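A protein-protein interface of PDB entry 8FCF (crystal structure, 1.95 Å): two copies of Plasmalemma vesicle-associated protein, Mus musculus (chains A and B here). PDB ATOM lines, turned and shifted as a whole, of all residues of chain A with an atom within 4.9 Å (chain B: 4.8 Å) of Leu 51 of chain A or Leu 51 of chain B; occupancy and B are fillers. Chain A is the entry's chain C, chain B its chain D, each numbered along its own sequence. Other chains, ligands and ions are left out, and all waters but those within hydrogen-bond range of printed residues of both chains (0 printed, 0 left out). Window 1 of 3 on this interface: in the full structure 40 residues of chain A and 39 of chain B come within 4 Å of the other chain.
OD2 of Asp 47 of chain A lies within salt-bridge range of NZ of Lys 48 of chain B (3.6 Å).
Among the printed residues, pairs that only touch across the chains: Gly 54 of chain A with Lys 55 of chain B (3.5 Å), Lys 55 of chain A with Lys 55 of chain B (3.6 Å), Lys 48 of chain A with Leu 51 of chain B (3.7 Å), Leu 51 of chain A with Lys 55 of chain B (3.8 Å), Lys 48 of chain A with Asp 47 of chain B (3.8 Å), Leu 51 of chain A with Leu 52 of chain B (3.8 Å), Leu 51 of chain A with Lys 48 of chain B (3.9 Å), Leu 51 of chain A with Leu 51 of chain B (3.9 Å) and Lys 55 of chain A with Gly 54 of chain B (3.9 Å).
Glu 49 of chain A touches none of the printed residues of chain B. Printed residues of chain B within 4 Å of Gly 54 of chain A: Lys 55. Printed residues of chain B within 4 Å of Lys 55 of chain A: Gly 54 and Lys 55. Ser 50 of chain B touches none of the printed residues of chain A. Of the printed residues of chain A, Leu 52 of chain B touches Leu 51 (3.8 Å). The nearest printed residue of chain B that does not touch Leu 51 of chain A is Asp 47 of chain B (5.7 Å). The nearest residue of chain A that does not touch Leu 51 of chain B is Leu 52 of chain A (4.5 Å). The nearest printed residue of chain A that does not touch Gly 54 of chain B is Leu 51 of chain A (7.6 Å).
Of the 9 printed residues of chain A, 5 touch a printed residue of chain B. Along chain B the printed residues that touch a printed residue of chain A span positions 47 to 55. Among the printed residues, 10 pairs touch across the chains. Among the printed residues, Asp or Glu carboxylates within 4 Å of a Lys or Arg side-chain nitrogen of the other chain: Asp 47 of chain A with Lys 48 of chain B (3.6 Å).
Asp 47 of chain A touches Lys 48 of chain B, and with the chains exchanged Lys 48 of chain A touches Asp 47 of chain B. Lys 48 of chain A touches Leu 51 of chain B, and with the chains exchanged Leu 51 of chain A touches Lys 48 of chain B. Leu 51 of chain B touches its own counterpart, Leu 51 of chain A. Leu 51 of chain A touches Leu 52 of chain B, but with the chains exchanged Leu 52 of chain A does not touch Leu 51 of chain B (4.5 Å). Positions printed for both chains: 47, 48, 49, 50, 51, 52, 53, 54 and 55.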
ATOM      1  N   ASP A  47     -16.250  -7.809   5.714  1.00  0.00           N
ATOM      2  CA  ASP A  47     -14.928  -7.314   5.329  1.00  0.00           C
ATOM      3  C   ASP A  47     -14.744  -7.416   3.802  1.00  0.00           C
ATOM      4  O   ASP A  47     -14.176  -6.501   3.221  1.00  0.00           O
ATOM      5  CB  ASP A  47     -13.798  -8.098   6.035  1.00  0.00           C
ATOM      6  CG  ASP A  47     -13.649  -7.848   7.526  1.00  0.00           C
ATOM      7  OD1 ASP A  47     -14.485  -7.099   8.094  1.00  0.00           O
ATOM      8  OD2 ASP A  47     -12.705  -8.415   8.132  1.00  0.00           O
ATOM      9  N   LYS A  48     -15.220  -8.517   3.161  1.00  0.00           N
ATOM     10  CA  LYS A  48     -15.106  -8.700   1.698  1.00  0.00           C
ATOM     11  C   LYS A  48     -15.990  -7.727   0.919  1.00  0.00           C
ATOM     12  O   LYS A  48     -15.592  -7.282  -0.149  1.00  0.00           O
ATOM     13  CB  LYS A  48     -15.433 -10.142   1.255  1.00  0.00           C
ATOM     14  CG  LYS A  48     -14.298 -11.126   1.530  1.00  0.00           C
ATOM     15  CD  LYS A  48     -14.543 -12.528   0.964  1.00  0.00           C
ATOM     16  CE  LYS A  48     -15.559 -13.352   1.723  1.00  0.00           C
ATOM     17  NZ  LYS A  48     -16.746 -13.694   0.897  1.00  0.00           N
ATOM     18  N   GLU A  49     -17.199  -7.433   1.419  1.00  0.00           N
ATOM     19  CA  GLU A  49     -18.097  -6.493   0.753  1.00  0.00           C
ATOM     20  C   GLU A  49     -17.469  -5.108   0.831  1.00  0.00           C
ATOM     21  O   GLU A  49     -17.543  -4.350  -0.142  1.00  0.00           O
ATOM     22  CB  GLU A  49     -19.502  -6.492   1.398  1.00  0.00           C
ATOM     23  CG  GLU A  49     -20.327  -5.250   1.075  1.00  0.00           C
ATOM     24  CD  GLU A  49     -21.789  -5.321   1.465  1.00  0.00           C
ATOM     25  OE1 GLU A  49     -22.097  -5.939   2.508  1.00  0.00           O
ATOM     26  OE2 GLU A  49     -22.625  -4.723   0.751  1.00  0.00           O
ATOM     27  N   SER A  50     -16.810  -4.804   1.961  1.00  0.00           N
ATOM     28  CA  SER A  50     -16.152  -3.518   2.167  1.00  0.00           C
ATOM     29  C   SER A  50     -14.969  -3.362   1.203  1.00  0.00           C
ATOM     30  O   SER A  50     -14.826  -2.299   0.599  1.00  0.00           O
ATOM     31  CB  SER A  50     -15.687  -3.377   3.616  1.00  0.00           C
ATOM     32  OG  SER A  50     -15.454  -2.026   3.954  1.00  0.00           O
ATOM     33  N   LEU A  51     -14.126  -4.410   1.055  1.00  0.00           N
ATOM     34  CA  LEU A  51     -12.974  -4.378   0.140  1.00  0.00           C
ATOM     35  C   LEU A  51     -13.438  -4.296  -1.313  1.00  0.00           C
ATOM     36  O   LEU A  51     -12.845  -3.547  -2.087  1.00  0.00           O
ATOM     37  CB  LEU A  51     -12.062  -5.615   0.319  1.00  0.00           C
ATOM     38  CG  LEU A  51     -11.224  -5.675   1.599  1.00  0.00           C
ATOM     39  CD1 LEU A  51     -10.543  -7.039   1.739  1.00  0.00           C
ATOM     40  CD2 LEU A  51     -10.193  -4.562   1.653  1.00  0.00           C
ATOM     41  N   LEU A  52     -14.511  -5.037  -1.676  1.00  0.00           N
ATOM     42  CA  LEU A  52     -15.051  -4.994  -3.041  1.00  0.00           C
ATOM     43  C   LEU A  52     -15.543  -3.572  -3.359  1.00  0.00           C
ATOM     44  O   LEU A  52     -15.227  -3.049  -4.419  1.00  0.00           O
ATOM     45  CB  LEU A  52     -16.216  -5.988  -3.249  1.00  0.00           C
ATOM     46  CG  LEU A  52     -16.189  -6.915  -4.472  1.00  0.00           C
ATOM     47  CD1 LEU A  52     -17.594  -7.374  -4.810  1.00  0.00           C
ATOM     48  CD2 LEU A  52     -15.561  -6.271  -5.698  1.00  0.00           C
ATOM     49  N   ALA A  53     -16.308  -2.956  -2.441  1.00  0.00           N
ATOM     50  CA  ALA A  53     -16.829  -1.598  -2.627  1.00  0.00           C
ATOM     51  C   ALA A  53     -15.686  -0.580  -2.743  1.00  0.00           C
ATOM     52  O   ALA A  53     -15.785   0.379  -3.513  1.00  0.00           O
ATOM     53  CB  ALA A  53     -17.741  -1.221  -1.466  1.00  0.00           C
ATOM     54  N   GLY A  54     -14.614  -0.809  -1.984  1.00  0.00           N
ATOM     55  CA  GLY A  54     -13.436   0.045  -1.988  1.00  0.00           C
ATOM     56  C   GLY A  54     -12.679  -0.047  -3.291  1.00  0.00           C
ATOM     57  O   GLY A  54     -12.295   0.987  -3.822  1.00  0.00           O
ATOM     58  N   LYS A  55     -12.439  -1.260  -3.828  1.00  0.00           N
ATOM     59  CA  LYS A  55     -11.717  -1.346  -5.104  1.00  0.00           C
ATOM     60  C   LYS A  55     -12.574  -0.838  -6.284  1.00  0.00           C
ATOM     61  O   LYS A  55     -12.015  -0.258  -7.212  1.00  0.00           O
ATOM     62  CB  LYS A  55     -11.108  -2.733  -5.374  1.00  0.00           C
ATOM     63  CG  LYS A  55     -12.072  -3.864  -5.677  1.00  0.00           C
ATOM     64  CD  LYS A  55     -11.783  -4.554  -7.001  1.00  0.00           C
ATOM     65  CE  LYS A  55     -10.430  -5.218  -7.139  1.00  0.00           C
ATOM     66  NZ  LYS A  55     -10.303  -5.919  -8.450  1.00  0.00           N
ATOM     67  N   ASP B  47      -9.085 -15.007   0.240  1.00  0.00           N
ATOM     68  CA  ASP B  47      -9.977 -14.115  -0.522  1.00  0.00           C
ATOM     69  C   ASP B  47      -9.674 -12.640  -0.237  1.00  0.00           C
ATOM     70  O   ASP B  47      -9.693 -11.841  -1.168  1.00  0.00           O
ATOM     71  CB  ASP B  47     -11.458 -14.387  -0.212  1.00  0.00           C
ATOM     72  CG  ASP B  47     -12.015 -15.691  -0.756  1.00  0.00           C
ATOM     73  OD1 ASP B  47     -11.229 -16.483  -1.339  1.00  0.00           O
ATOM     74  OD2 ASP B  47     -13.237 -15.927  -0.594  1.00  0.00           O
ATOM     75  N   LYS B  48      -9.446 -12.272   1.034  1.00  0.00           N
ATOM     76  CA  LYS B  48      -9.152 -10.888   1.378  1.00  0.00           C
ATOM     77  C   LYS B  48      -7.726 -10.492   0.939  1.00  0.00           C
ATOM     78  O   LYS B  48      -7.510  -9.335   0.613  1.00  0.00           O
ATOM     79  CB  LYS B  48      -9.453 -10.591   2.858  1.00  0.00           C
ATOM     80  CG  LYS B  48      -8.503 -11.179   3.892  1.00  0.00           C
ATOM     81  CD  LYS B  48      -8.853 -10.696   5.310  1.00  0.00           C
ATOM     82  CE  LYS B  48     -10.265 -11.027   5.743  1.00  0.00           C
ATOM     83  NZ  LYS B  48     -10.424 -11.010   7.225  1.00  0.00           N
ATOM     84  N   GLU B  49      -6.784 -11.446   0.876  1.00  0.00           N
ATOM     85  CA  GLU B  49      -5.421 -11.215   0.374  1.00  0.00           C
ATOM     86  C   GLU B  49      -5.504 -10.894  -1.149  1.00  0.00           C
ATOM     87  O   GLU B  49      -4.790 -10.013  -1.638  1.00  0.00           O
ATOM     88  CB  GLU B  49      -4.548 -12.465   0.641  1.00  0.00           C
ATOM     89  CG  GLU B  49      -3.099 -12.390   0.168  1.00  0.00           C
ATOM     90  CD  GLU B  49      -2.526 -13.688  -0.379  1.00  0.00           C
ATOM     91  OE1 GLU B  49      -3.162 -14.298  -1.269  1.00  0.00           O
ATOM     92  OE2 GLU B  49      -1.424 -14.081   0.066  1.00  0.00           O
ATOM     93  N   SER B  50      -6.406 -11.591  -1.869  1.00  0.00           N
ATOM     94  CA  SER B  50      -6.665 -11.418  -3.306  1.00  0.00           C
ATOM     95  C   SER B  50      -7.325 -10.052  -3.592  1.00  0.00           C
ATOM     96  O   SER B  50      -6.903  -9.351  -4.518  1.00  0.00           O
ATOM     97  CB  SER B  50      -7.544 -12.556  -3.819  1.00  0.00           C
ATOM     98  OG  SER B  50      -7.471 -12.685  -5.225  1.00  0.00           O
ATOM     99  N   LEU B  51      -8.340  -9.668  -2.783  1.00  0.00           N
ATOM    100  CA  LEU B  51      -9.017  -8.371  -2.910  1.00  0.00           C
ATOM    101  C   LEU B  51      -8.068  -7.228  -2.559  1.00  0.00           C
ATOM    102  O   LEU B  51      -8.079  -6.223  -3.247  1.00  0.00           O
ATOM    103  CB  LEU B  51     -10.276  -8.282  -2.017  1.00  0.00           C
ATOM    104  CG  LEU B  51     -11.480  -9.139  -2.431  1.00  0.00           C
ATOM    105  CD1 LEU B  51     -12.565  -9.113  -1.363  1.00  0.00           C
ATOM    106  CD2 LEU B  51     -12.053  -8.687  -3.774  1.00  0.00           C
ATOM    107  N   LEU B  52      -7.247  -7.379  -1.507  1.00  0.00           N
ATOM    108  CA  LEU B  52      -6.258  -6.363  -1.133  1.00  0.00           C
ATOM    109  C   LEU B  52      -5.223  -6.154  -2.250  1.00  0.00           C
ATOM    110  O   LEU B  52      -4.910  -5.013  -2.569  1.00  0.00           O
ATOM    111  CB  LEU B  52      -5.546  -6.723   0.184  1.00  0.00           C
ATOM    112  CG  LEU B  52      -6.303  -6.365   1.455  1.00  0.00           C
ATOM    113  CD1 LEU B  52      -5.655  -7.011   2.675  1.00  0.00           C
ATOM    114  CD2 LEU B  52      -6.392  -4.852   1.644  1.00  0.00           C
ATOM    115  N   ALA B  53      -4.715  -7.241  -2.849  1.00  0.00           N
ATOM    116  CA  ALA B  53      -3.758  -7.160  -3.958  1.00  0.00           C
ATOM    117  C   ALA B  53      -4.393  -6.482  -5.177  1.00  0.00           C
ATOM    118  O   ALA B  53      -3.712  -5.742  -5.888  1.00  0.00           O
ATOM    119  CB  ALA B  53      -3.266  -8.546  -4.337  1.00  0.00           C
ATOM    120  N   GLY B  54      -5.683  -6.737  -5.400  1.00  0.00           N
ATOM    121  CA  GLY B  54      -6.434  -6.112  -6.481  1.00  0.00           C
ATOM    122  C   GLY B  54      -6.627  -4.626  -6.254  1.00  0.00           C
ATOM    123  O   GLY B  54      -6.410  -3.821  -7.163  1.00  0.00           O
ATOM    124  N   LYS B  55      -6.981  -4.259  -5.007  1.00  0.00           N
ATOM    125  CA  LYS B  55      -7.177  -2.877  -4.581  1.00  0.00           C
ATOM    126  C   LYS B  55      -5.860  -2.119  -4.629  1.00  0.00           C
ATOM    127  O   LYS B  55      -5.852  -0.974  -5.078  1.00  0.00           O
ATOM    128  CB  LYS B  55      -7.751  -2.823  -3.151  1.00  0.00           C
ATOM    129  CG  LYS B  55      -8.387  -1.485  -2.783  1.00  0.00           C
ATOM    130  CD  LYS B  55      -8.715  -1.394  -1.287  1.00  0.00           C
ATOM    131  CE  LYS B  55     -10.175  -1.123  -1.025  1.00  0.00           C
ATOM    132  NZ  LYS B  55     -10.470  -0.937   0.428  1.00  0.00           N
